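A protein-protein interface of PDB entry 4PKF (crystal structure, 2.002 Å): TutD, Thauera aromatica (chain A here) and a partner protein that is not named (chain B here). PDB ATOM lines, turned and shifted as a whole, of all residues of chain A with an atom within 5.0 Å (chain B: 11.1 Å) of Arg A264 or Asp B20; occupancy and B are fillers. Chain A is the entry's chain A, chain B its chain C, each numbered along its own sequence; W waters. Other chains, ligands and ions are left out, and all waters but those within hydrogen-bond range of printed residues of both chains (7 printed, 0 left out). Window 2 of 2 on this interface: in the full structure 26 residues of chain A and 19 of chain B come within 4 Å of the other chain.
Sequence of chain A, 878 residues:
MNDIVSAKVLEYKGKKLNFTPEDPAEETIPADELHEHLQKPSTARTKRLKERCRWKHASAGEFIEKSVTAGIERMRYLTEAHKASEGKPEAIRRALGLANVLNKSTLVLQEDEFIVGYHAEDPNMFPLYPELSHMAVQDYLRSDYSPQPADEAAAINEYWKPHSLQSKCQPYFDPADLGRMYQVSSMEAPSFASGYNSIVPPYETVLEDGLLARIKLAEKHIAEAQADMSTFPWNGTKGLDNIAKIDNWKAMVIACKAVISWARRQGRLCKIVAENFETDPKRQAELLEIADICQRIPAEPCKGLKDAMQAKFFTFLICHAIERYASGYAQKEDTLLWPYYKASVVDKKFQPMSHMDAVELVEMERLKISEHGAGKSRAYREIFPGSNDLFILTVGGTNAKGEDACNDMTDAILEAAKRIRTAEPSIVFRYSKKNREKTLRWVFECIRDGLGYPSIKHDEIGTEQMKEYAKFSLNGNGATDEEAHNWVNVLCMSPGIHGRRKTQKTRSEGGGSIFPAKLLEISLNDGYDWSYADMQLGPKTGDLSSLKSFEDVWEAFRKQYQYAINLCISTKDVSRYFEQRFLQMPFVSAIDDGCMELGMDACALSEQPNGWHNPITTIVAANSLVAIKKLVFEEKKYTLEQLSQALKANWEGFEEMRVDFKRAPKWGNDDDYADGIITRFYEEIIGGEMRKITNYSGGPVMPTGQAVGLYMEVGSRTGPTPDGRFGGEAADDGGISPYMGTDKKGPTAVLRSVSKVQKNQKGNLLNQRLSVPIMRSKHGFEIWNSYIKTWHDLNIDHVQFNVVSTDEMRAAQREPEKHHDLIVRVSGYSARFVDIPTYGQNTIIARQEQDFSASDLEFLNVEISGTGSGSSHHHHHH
The side-chain carboxylate (OD2) of Asp B20 lies within salt-bridge range of the guanidinium group (NH1) of Arg A264. The side-chain carboxylate (OD2) of Asp B21 lies within salt-bridge range of the guanidinium group (NH1) of Arg A268. The guanidinium group (NE) of Arg A268 lies within salt-bridge range of the side-chain carboxylate (OD2) of Asp B28 (2.7 Å).
NE of Arg A264 is in hydrogen-bond range of O of Gln A295. The backbone NH (N) of Val B15 lies within hydrogen-bond range of the backbone carbonyl oxygen (O) of Lys B26, at 3.0 Å. The side-chain carboxylate (OD2) of Asp B21 is in salt-bridge range of the side-chain amino group (NZ) of Lys B26.
OD2 of Asp B20 touches CG2 of Ile A260, at 3.4 Å. CB of Ser A261 touches CB of Asp B20, 3.9 Å away. CB of Asp B21 touches OG of Ser A261, at 3.4 Å. Asp B21 touches Arg A265 (OD2 to CD, 3.6 Å). Arg A265 touches Ser B43 (NH1 to O, 3.6 Å). Arg A265 touches Pro B45 (NH1 to CG, 3.3 Å). Arg A268 touches Val B15 (NH1 to CG2, 3.7 Å). Arg A268 touches Pro B16. NH2 of Arg A268 touches CB of Ala B19 (3.7 Å).
Arg A264 touches just one residue of chain B: Asp B20. Of chain A, only Ile A260, Ser A261 and Arg A264 come within 4 Å of Asp B20. Of chain B, only Asp B20 (3.4 Å) comes within 4 Å of Ile A260. Of the printed residues of chain B, Ser A261 touches Asp B20 and Asp B21. Arg A268 touches five residues of chain B. No residue of chain B comes within 4 Å of Cys A294. No residue of chain B comes within 4 Å of Gln A295. No residue of chain B comes within 4 Å of Ala A299. Of the printed residues of chain A, Ser B43 touches Arg A265 (3.6 Å). Printed residues of chain A within 4 Å of Pro B16: Arg A268. Of the printed residues of chain A, Pro B45 touches Arg A265 (3.3 Å). Printed residues of chain A within 4 Å of Asp B21: Ser A261, Arg A265 and Arg A268. Printed residues of chain A within 4 Å of Ala B19: Arg A268. The nearest residue of chain B that does not touch Arg A264 is Asp B21 (6.0 Å). The nearest printed residue of chain A that does not touch Asp B21 is Arg A264 (6.0 Å).
Hydrophobic or aromatic side chains of chain A that line the printed part of chain B: Ile A260. Of the 16 printed residues of chain B, 8 touch a printed residue of chain A. Printed residues of chain B that touch a printed residue of chain A: Val B15, Pro B16, Ala B19, Asp B20, Asp B21, Asp B28, Ser B43 and Pro B45.
Water W3 lies within hydrogen-bond range of OD2 of Asp B28 (2.6 Å), O of Pro B14 (3.2 Å) and NE of Arg A268 (3.2 Å). Water W1 bridges the side-chain carboxylate of Asp B21 (2.7 Å) and the backbone carbonyl oxygen of Ser A261 (2.8 Å). Water W2 lies within hydrogen-bond range of the side-chain amino group (NZ) of Lys B26 (2.8 Å), the guanidinium group (NE) of Arg A265 (3.4 Å) and the side-chain carboxylate (OD2) of Asp B21 (3.4 Å). Water W7 lies within hydrogen-bond range of OG of Ser B43 (2.8 Å), O of Arg A265 (2.9 Å) and OD2 of Asp B28 (3.2 Å). Water W6 lies within hydrogen-bond range of OD1 of Asp B20 (2.9 Å), NE2 of Gln A295 (3.1 Å) and NH1 of Arg A264 (3.4 Å). Water W4 lies within hydrogen-bond range of the side-chain carboxylate (OD1) of Asp B20 (3.3 Å) and the guanidinium group (NH1) of Arg A264 (3.4 Å).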
ATOM      1  N   LEU A 212       1.159  28.800  -0.649  1.00  0.00           N
ATOM      2  CA  LEU A 212      -0.169  28.798  -0.023  1.00  0.00           C
ATOM      3  C   LEU A 212      -1.223  28.815  -1.123  1.00  0.00           C
ATOM      4  O   LEU A 212      -2.198  28.096  -1.046  1.00  0.00           O
ATOM      5  CB  LEU A 212      -0.342  29.990   0.925  1.00  0.00           C
ATOM      6  CG  LEU A 212       0.254  29.922   2.334  1.00  0.00           C
ATOM      7  CD1 LEU A 212       0.173  31.343   3.046  1.00  0.00           C
ATOM      8  CD2 LEU A 212      -0.440  28.837   3.157  1.00  0.00           C
ATOM      9  N   VAL A 259       6.843  21.776   2.859  1.00  0.00           N
ATOM     10  CA  VAL A 259       7.890  22.708   2.426  1.00  0.00           C
ATOM     11  C   VAL A 259       7.745  24.042   3.190  1.00  0.00           C
ATOM     12  O   VAL A 259       8.747  24.584   3.703  1.00  0.00           O
ATOM     13  CB  VAL A 259       7.866  22.946   0.902  1.00  0.00           C
ATOM     14  CG1 VAL A 259       8.816  24.124   0.514  1.00  0.00           C
ATOM     15  CG2 VAL A 259       8.322  21.670   0.129  1.00  0.00           C
ATOM     16  N   ILE A 260       6.513  24.560   3.297  1.00  0.00           N
ATOM     17  CA  ILE A 260       6.266  25.791   4.069  1.00  0.00           C
ATOM     18  C   ILE A 260       6.706  25.629   5.510  1.00  0.00           C
ATOM     19  O   ILE A 260       7.378  26.496   6.100  1.00  0.00           O
ATOM     20  CB  ILE A 260       4.777  26.183   4.036  1.00  0.00           C
ATOM     21  CG1 ILE A 260       4.400  26.639   2.626  1.00  0.00           C
ATOM     22  CG2 ILE A 260       4.469  27.298   5.064  1.00  0.00           C
ATOM     23  CD1 ILE A 260       2.896  26.988   2.428  1.00  0.00           C
ATOM     24  N   SER A 261       6.320  24.512   6.098  1.00  0.00           N
ATOM     25  CA  SER A 261       6.658  24.271   7.486  1.00  0.00           C
ATOM     26  C   SER A 261       8.179  24.228   7.709  1.00  0.00           C
ATOM     27  O   SER A 261       8.704  24.772   8.696  1.00  0.00           O
ATOM     28  CB  SER A 261       6.010  22.978   7.953  1.00  0.00           C
ATOM     29  OG  SER A 261       6.459  22.676   9.247  1.00  0.00           O
ATOM     30  N   TRP A 262       8.880  23.605   6.765  1.00  0.00           N
ATOM     31  CA  TRP A 262      10.326  23.483   6.816  1.00  0.00           C
ATOM     32  C   TRP A 262      11.020  24.866   6.653  1.00  0.00           C
ATOM     33  O   TRP A 262      11.949  25.183   7.374  1.00  0.00           O
ATOM     34  CB  TRP A 262      10.745  22.479   5.737  1.00  0.00           C
ATOM     35  CG  TRP A 262      12.204  22.386   5.289  1.00  0.00           C
ATOM     36  CD1 TRP A 262      13.197  21.646   5.862  1.00  0.00           C
ATOM     37  CD2 TRP A 262      12.745  22.907   4.078  1.00  0.00           C
ATOM     38  NE1 TRP A 262      14.343  21.708   5.100  1.00  0.00           N
ATOM     39  CE2 TRP A 262      14.086  22.472   3.994  1.00  0.00           C
ATOM     40  CE3 TRP A 262      12.221  23.694   3.047  1.00  0.00           C
ATOM     41  CZ2 TRP A 262      14.923  22.811   2.925  1.00  0.00           C
ATOM     42  CZ3 TRP A 262      13.064  24.039   1.976  1.00  0.00           C
ATOM     43  CH2 TRP A 262      14.395  23.580   1.924  1.00  0.00           C
ATOM     44  N   ALA A 263      10.541  25.678   5.722  1.00  0.00           N
ATOM     45  CA  ALA A 263      11.072  27.020   5.524  1.00  0.00           C
ATOM     46  C   ALA A 263      10.903  27.845   6.805  1.00  0.00           C
ATOM     47  O   ALA A 263      11.813  28.584   7.243  1.00  0.00           O
ATOM     48  CB  ALA A 263      10.356  27.701   4.371  1.00  0.00           C
ATOM     49  N   ARG A 264       9.726  27.712   7.406  1.00  0.00           N
ATOM     50  CA  ARG A 264       9.424  28.513   8.570  1.00  0.00           C
ATOM     51  C   ARG A 264      10.232  28.042   9.761  1.00  0.00           C
ATOM     52  O   ARG A 264      10.644  28.852  10.587  1.00  0.00           O
ATOM     53  CB  ARG A 264       7.937  28.494   8.836  1.00  0.00           C
ATOM     54  CG  ARG A 264       7.207  29.313   7.818  1.00  0.00           C
ATOM     55  CD  ARG A 264       5.686  29.149   8.009  1.00  0.00           C
ATOM     56  NE  ARG A 264       5.042  30.246   7.307  1.00  0.00           N
ATOM     57  CZ  ARG A 264       3.751  30.324   7.022  1.00  0.00           C
ATOM     58  NH1 ARG A 264       2.931  29.347   7.363  1.00  0.00           N
ATOM     59  NH2 ARG A 264       3.281  31.404   6.405  1.00  0.00           N
ATOM     60  N   ARG A 265      10.548  26.755   9.803  1.00  0.00           N
ATOM     61  CA  ARG A 265      11.388  26.216  10.874  1.00  0.00           C
ATOM     62  C   ARG A 265      12.860  26.653  10.698  1.00  0.00           C
ATOM     63  O   ARG A 265      13.617  26.825  11.677  1.00  0.00           O
ATOM     64  CB  ARG A 265      11.261  24.686  10.914  1.00  0.00           C
ATOM     65  CG  ARG A 265      11.944  24.031  12.104  1.00  0.00           C
ATOM     66  CD  ARG A 265      11.397  22.639  12.346  1.00  0.00           C
ATOM     67  NE  ARG A 265      11.753  21.724  11.265  1.00  0.00           N
ATOM     68  CZ  ARG A 265      12.905  21.045  11.180  1.00  0.00           C
ATOM     69  NH1 ARG A 265      13.842  21.132  12.117  1.00  0.00           N
ATOM     70  NH2 ARG A 265      13.114  20.247  10.145  1.00  0.00           N
ATOM     71  N   GLN A 266      13.263  26.813   9.442  1.00  0.00           N
ATOM     72  CA  GLN A 266      14.571  27.383   9.121  1.00  0.00           C
ATOM     73  C   GLN A 266      14.609  28.815   9.639  1.00  0.00           C
ATOM     74  O   GLN A 266      15.581  29.244  10.289  1.00  0.00           O
ATOM     75  CB  GLN A 266      14.832  27.334   7.603  1.00  0.00           C
ATOM     76  CG  GLN A 266      16.212  27.910   7.223  1.00  0.00           C
ATOM     77  CD  GLN A 266      17.317  26.896   7.475  1.00  0.00           C
ATOM     78  OE1 GLN A 266      17.161  25.717   7.169  1.00  0.00           O
ATOM     79  NE2 GLN A 266      18.422  27.343   8.045  1.00  0.00           N
ATOM     80  N   GLY A 267      13.532  29.544   9.356  1.00  0.00           N
ATOM     81  CA  GLY A 267      13.341  30.890   9.848  1.00  0.00           C
ATOM     82  C   GLY A 267      13.438  30.987  11.361  1.00  0.00           C
ATOM     83  O   GLY A 267      14.040  31.929  11.896  1.00  0.00           O
ATOM     84  N   ARG A 268      12.853  30.013  12.055  1.00  0.00           N
ATOM     85  CA  ARG A 268      12.816  30.020  13.509  1.00  0.00           C
ATOM     86  C   ARG A 268      14.207  29.805  14.099  1.00  0.00           C
ATOM     87  O   ARG A 268      14.525  30.369  15.138  1.00  0.00           O
ATOM     88  CB  ARG A 268      11.846  28.950  14.013  1.00  0.00           C
ATOM     89  CG  ARG A 268      11.739  28.873  15.493  1.00  0.00           C
ATOM     90  CD  ARG A 268      10.444  28.112  15.879  1.00  0.00           C
ATOM     91  NE  ARG A 268      10.605  26.649  15.737  1.00  0.00           N
ATOM     92  CZ  ARG A 268       9.823  25.864  15.003  1.00  0.00           C
ATOM     93  NH1 ARG A 268      10.047  24.552  14.969  1.00  0.00           N
ATOM     94  NH2 ARG A 268       8.817  26.376  14.312  1.00  0.00           N
ATOM     95  N   CYS A 294      11.926  34.144   5.738  1.00  0.00           N
ATOM     96  CA  CYS A 294      11.623  32.713   5.765  1.00  0.00           C
ATOM     97  C   CYS A 294      10.196  32.403   6.258  1.00  0.00           C
ATOM     98  O   CYS A 294       9.585  31.371   5.900  1.00  0.00           O
ATOM     99  CB  CYS A 294      12.620  31.995   6.656  1.00  0.00           C
ATOM    100  SG  CYS A 294      14.263  31.822   5.929  1.00  0.00           S
ATOM    101  N   GLN A 295       9.677  33.274   7.112  1.00  0.00           N
ATOM    102  CA  GLN A 295       8.298  33.141   7.567  1.00  0.00           C
ATOM    103  C   GLN A 295       7.316  33.379   6.421  1.00  0.00           C
ATOM    104  O   GLN A 295       6.315  32.675   6.298  1.00  0.00           O
ATOM    105  CB  GLN A 295       8.002  34.141   8.698  1.00  0.00           C
ATOM    106  CG  GLN A 295       6.588  33.990   9.281  1.00  0.00           C
ATOM    107  CD  GLN A 295       6.395  32.622   9.938  1.00  0.00           C
ATOM    108  OE1 GLN A 295       7.375  31.942  10.312  1.00  0.00           O
ATOM    109  NE2 GLN A 295       5.146  32.204  10.067  1.00  0.00           N
ATOM    110  N   ALA A 299       5.787  30.624   1.359  1.00  0.00           N
ATOM    111  CA  ALA A 299       4.340  30.534   1.572  1.00  0.00           C
ATOM    112  C   ALA A 299       3.588  31.542   0.712  1.00  0.00           C
ATOM    113  O   ALA A 299       2.621  31.190   0.023  1.00  0.00           O
ATOM    114  CB  ALA A 299       3.998  30.742   3.079  1.00  0.00           C
ATOM    115  N   PRO B  14      11.059  25.062  23.135  1.00  0.00           N
ATOM    116  CA  PRO B  14       9.696  24.606  22.825  1.00  0.00           C
ATOM    117  C   PRO B  14       9.190  25.246  21.548  1.00  0.00           C
ATOM    118  O   PRO B  14       9.391  26.439  21.337  1.00  0.00           O
ATOM    119  CB  PRO B  14       8.864  25.083  24.040  1.00  0.00           C
ATOM    120  CG  PRO B  14       9.853  25.133  25.160  1.00  0.00           C
ATOM    121  CD  PRO B  14      11.160  25.599  24.508  1.00  0.00           C
ATOM    122  N   VAL B  15       8.561  24.460  20.693  1.00  0.00           N
ATOM    123  CA  VAL B  15       8.017  24.991  19.437  1.00  0.00           C
ATOM    124  C   VAL B  15       6.836  25.877  19.743  1.00  0.00           C
ATOM    125  O   VAL B  15       5.942  25.427  20.442  1.00  0.00           O
ATOM    126  CB  VAL B  15       7.543  23.858  18.485  1.00  0.00           C
ATOM    127  CG1 VAL B  15       6.810  24.437  17.265  1.00  0.00           C
ATOM    128  CG2 VAL B  15       8.739  22.976  18.066  1.00  0.00           C
ATOM    129  N   PRO B  16       6.833  27.121  19.223  1.00  0.00           N
ATOM    130  CA  PRO B  16       5.696  28.038  19.362  1.00  0.00           C
ATOM    131  C   PRO B  16       4.398  27.317  19.019  1.00  0.00           C
ATOM    132  O   PRO B  16       4.320  26.626  18.004  1.00  0.00           O
ATOM    133  CB  PRO B  16       5.993  29.141  18.354  1.00  0.00           C
ATOM    134  CG  PRO B  16       7.554  29.154  18.252  1.00  0.00           C
ATOM    135  CD  PRO B  16       7.958  27.708  18.453  1.00  0.00           C
ATOM    136  N   LYS B  17       3.380  27.482  19.854  1.00  0.00           N
ATOM    137  CA  LYS B  17       2.201  26.645  19.726  1.00  0.00           C
ATOM    138  C   LYS B  17       1.389  27.016  18.489  1.00  0.00           C
ATOM    139  O   LYS B  17       0.554  26.238  18.035  1.00  0.00           O
ATOM    140  CB  LYS B  17       1.370  26.731  21.020  1.00  0.00           C
ATOM    141  CG  LYS B  17       2.008  25.896  22.141  1.00  0.00           C
ATOM    142  CD  LYS B  17       1.227  25.955  23.413  1.00  0.00           C
ATOM    143  CE  LYS B  17       1.613  24.887  24.405  1.00  0.00           C
ATOM    144  NZ  LYS B  17       3.014  24.411  24.244  1.00  0.00           N
ATOM    145  N   ASP B  18       1.661  28.185  17.914  1.00  0.00           N
ATOM    146  CA  ASP B  18       1.024  28.572  16.650  1.00  0.00           C
ATOM    147  C   ASP B  18       1.869  28.238  15.385  1.00  0.00           C
ATOM    148  O   ASP B  18       1.533  28.665  14.278  1.00  0.00           O
ATOM    149  CB  ASP B  18       0.713  30.062  16.664  1.00  0.00           C
ATOM    150  CG  ASP B  18       1.964  30.900  16.734  1.00  0.00           C
ATOM    151  OD1 ASP B  18       2.999  30.396  17.236  1.00  0.00           O
ATOM    152  OD2 ASP B  18       1.919  32.058  16.269  1.00  0.00           O
ATOM    153  N   ALA B  19       2.958  27.492  15.546  1.00  0.00           N
ATOM    154  CA  ALA B  19       3.794  27.111  14.391  1.00  0.00           C
ATOM    155  C   ALA B  19       3.121  26.022  13.570  1.00  0.00           C
ATOM    156  O   ALA B  19       2.372  25.209  14.109  1.00  0.00           O
ATOM    157  CB  ALA B  19       5.164  26.635  14.849  1.00  0.00           C
ATOM    158  N   ASP B  20       3.388  26.007  12.267  1.00  0.00           N
ATOM    159  CA  ASP B  20       2.894  24.941  11.394  1.00  0.00           C
ATOM    160  C   ASP B  20       3.305  23.541  11.881  1.00  0.00           C
ATOM    161  O   ASP B  20       2.612  22.566  11.649  1.00  0.00           O
ATOM    162  CB  ASP B  20       3.411  25.126   9.953  1.00  0.00           C
ATOM    163  CG  ASP B  20       2.965  26.445   9.318  1.00  0.00           C
ATOM    164  OD1 ASP B  20       2.416  27.318  10.033  1.00  0.00           O
ATOM    165  OD2 ASP B  20       3.174  26.608   8.090  1.00  0.00           O
ATOM    166  N   ASP B  21       4.460  23.422  12.519  1.00  0.00           N
ATOM    167  CA  ASP B  21       4.929  22.097  12.905  1.00  0.00           C
ATOM    168  C   ASP B  21       4.726  21.833  14.375  1.00  0.00           C
ATOM    169  O   ASP B  21       5.341  20.913  14.928  1.00  0.00           O
ATOM    170  CB  ASP B  21       6.410  21.928  12.578  1.00  0.00           C
ATOM    171  CG  ASP B  21       7.271  22.965  13.279  1.00  0.00           C
ATOM    172  OD1 ASP B  21       6.999  24.173  13.098  1.00  0.00           O
ATOM    173  OD2 ASP B  21       8.199  22.579  14.022  1.00  0.00           O
ATOM    174  N   TYR B  22       3.910  22.654  15.034  1.00  0.00           N
ATOM    175  CA  TYR B  22       3.662  22.414  16.452  1.00  0.00           C
ATOM    176  C   TYR B  22       2.926  21.090  16.687  1.00  0.00           C
ATOM    177  O   TYR B  22       1.930  20.797  16.051  1.00  0.00           O
ATOM    178  CB  TYR B  22       2.858  23.538  17.108  1.00  0.00           C
ATOM    179  CG  TYR B  22       2.478  23.162  18.524  1.00  0.00           C
ATOM    180  CD1 TYR B  22       3.441  23.126  19.522  1.00  0.00           C
ATOM    181  CD2 TYR B  22       1.169  22.831  18.856  1.00  0.00           C
ATOM    182  CE1 TYR B  22       3.122  22.753  20.827  1.00  0.00           C
ATOM    183  CE2 TYR B  22       0.828  22.465  20.166  1.00  0.00           C
ATOM    184  CZ  TYR B  22       1.821  22.431  21.145  1.00  0.00           C
ATOM    185  OH  TYR B  22       1.530  22.082  22.449  1.00  0.00           O
ATOM    186  N   GLU B  23       3.448  20.317  17.625  1.00  0.00           N
ATOM    187  CA  GLU B  23       2.777  19.155  18.204  1.00  0.00           C
ATOM    188  C   GLU B  23       3.108  19.199  19.688  1.00  0.00           C
ATOM    189  O   GLU B  23       4.170  19.711  20.070  1.00  0.00           O
ATOM    190  CB  GLU B  23       3.271  17.835  17.598  1.00  0.00           C
ATOM    191  CG  GLU B  23       3.082  17.704  16.107  1.00  0.00           C
ATOM    192  CD  GLU B  23       3.663  16.394  15.571  1.00  0.00           C
ATOM    193  OE1 GLU B  23       2.979  15.358  15.699  1.00  0.00           O
ATOM    194  OE2 GLU B  23       4.802  16.402  15.034  1.00  0.00           O
ATOM    195  N   ALA B  24       2.233  18.650  20.525  1.00  0.00           N
ATOM    196  CA  ALA B  24       2.426  18.747  21.974  1.00  0.00           C
ATOM    197  C   ALA B  24       3.735  18.100  22.415  1.00  0.00           C
ATOM    198  O   ALA B  24       4.053  16.995  21.995  1.00  0.00           O
ATOM    199  CB  ALA B  24       1.210  18.093  22.721  1.00  0.00           C
ATOM    200  N   LYS B  26       6.733  19.086  21.594  1.00  0.00           N
ATOM    201  CA  LYS B  26       7.784  19.232  20.580  1.00  0.00           C
ATOM    202  C   LYS B  26       8.694  20.430  20.856  1.00  0.00           C
ATOM    203  O   LYS B  26       8.218  21.503  21.237  1.00  0.00           O
ATOM    204  CB  LYS B  26       7.163  19.379  19.194  1.00  0.00           C
ATOM    205  CG  LYS B  26       8.120  19.129  17.974  1.00  0.00           C
ATOM    206  CD  LYS B  26       7.236  19.201  16.724  1.00  0.00           C
ATOM    207  CE  LYS B  26       7.878  18.717  15.464  1.00  0.00           C
ATOM    208  NZ  LYS B  26       8.754  19.798  14.897  1.00  0.00           N
ATOM    209  N   ASP B  28      12.681  22.491  19.502  1.00  0.00           N
ATOM    210  CA  ASP B  28      13.934  22.545  18.727  1.00  0.00           C
ATOM    211  C   ASP B  28      15.118  22.396  19.655  1.00  0.00           C
ATOM    212  O   ASP B  28      15.260  23.169  20.599  1.00  0.00           O
ATOM    213  CB  ASP B  28      14.103  23.863  17.971  1.00  0.00           C
ATOM    214  CG  ASP B  28      12.955  24.184  17.022  1.00  0.00           C
ATOM    215  OD1 ASP B  28      12.409  23.276  16.353  1.00  0.00           O
ATOM    216  OD2 ASP B  28      12.657  25.395  16.896  1.00  0.00           O
ATOM    217  N   SER B  43      19.665  22.719  14.238  1.00  0.00           N
ATOM    218  CA  SER B  43      18.346  22.679  14.894  1.00  0.00           C
ATOM    219  C   SER B  43      17.619  21.390  14.552  1.00  0.00           C
ATOM    220  O   SER B  43      17.186  21.220  13.419  1.00  0.00           O
ATOM    221  CB  SER B  43      17.464  23.864  14.482  1.00  0.00           C
ATOM    222  OG  SER B  43      16.168  23.754  15.089  1.00  0.00           O
ATOM    223  N   PRO B  45      14.459  18.682  15.618  1.00  0.00           N
ATOM    224  CA  PRO B  45      13.228  18.634  16.403  1.00  0.00           C
ATOM    225  C   PRO B  45      13.239  17.442  17.348  1.00  0.00           C
ATOM    226  O   PRO B  45      13.645  16.353  16.930  1.00  0.00           O
ATOM    227  CB  PRO B  45      12.121  18.477  15.339  1.00  0.00           C
ATOM    228  CG  PRO B  45      12.793  18.601  14.024  1.00  0.00           C
ATOM    229  CD  PRO B  45      14.226  18.231  14.240  1.00  0.00           C
ATOM    230  N   PHE B  47      11.243  15.564  21.176  1.00  0.00           N
ATOM    231  CA  PHE B  47      10.115  15.539  22.120  1.00  0.00           C
ATOM    232  C   PHE B  47      10.546  15.344  23.578  1.00  0.00           C
ATOM    233  O   PHE B  47      11.201  14.352  23.918  1.00  0.00           O
ATOM    234  CB  PHE B  47       9.131  14.449  21.722  1.00  0.00           C
ATOM    235  CG  PHE B  47       8.414  14.749  20.458  1.00  0.00           C
ATOM    236  CD1 PHE B  47       9.002  14.450  19.227  1.00  0.00           C
ATOM    237  CD2 PHE B  47       7.169  15.365  20.488  1.00  0.00           C
ATOM    238  CE1 PHE B  47       8.351  14.737  18.039  1.00  0.00           C
ATOM    239  CE2 PHE B  47       6.501  15.656  19.307  1.00  0.00           C
ATOM    240  CZ  PHE B  47       7.096  15.339  18.078  1.00  0.00           C
HETATM  241  O   HOH W   1       7.207  25.730  10.884  1.00  0.00           O
HETATM  242  O   HOH W   2       9.020  19.837  12.126  1.00  0.00           O
HETATM  243  O   HOH W   3      11.448  26.546  18.853  1.00  0.00           O
HETATM  244  O   HOH W   4       0.006  27.738   7.849  1.00  0.00           O
HETATM  245  O   HOH W   5      14.129  22.047  14.592  1.00  0.00           O
HETATM  246  O   HOH W   6       3.054  30.015  10.708  1.00  0.00           O
HETATM  247  O   HOH W   7      14.441  25.837  14.260  1.00  0.00           O
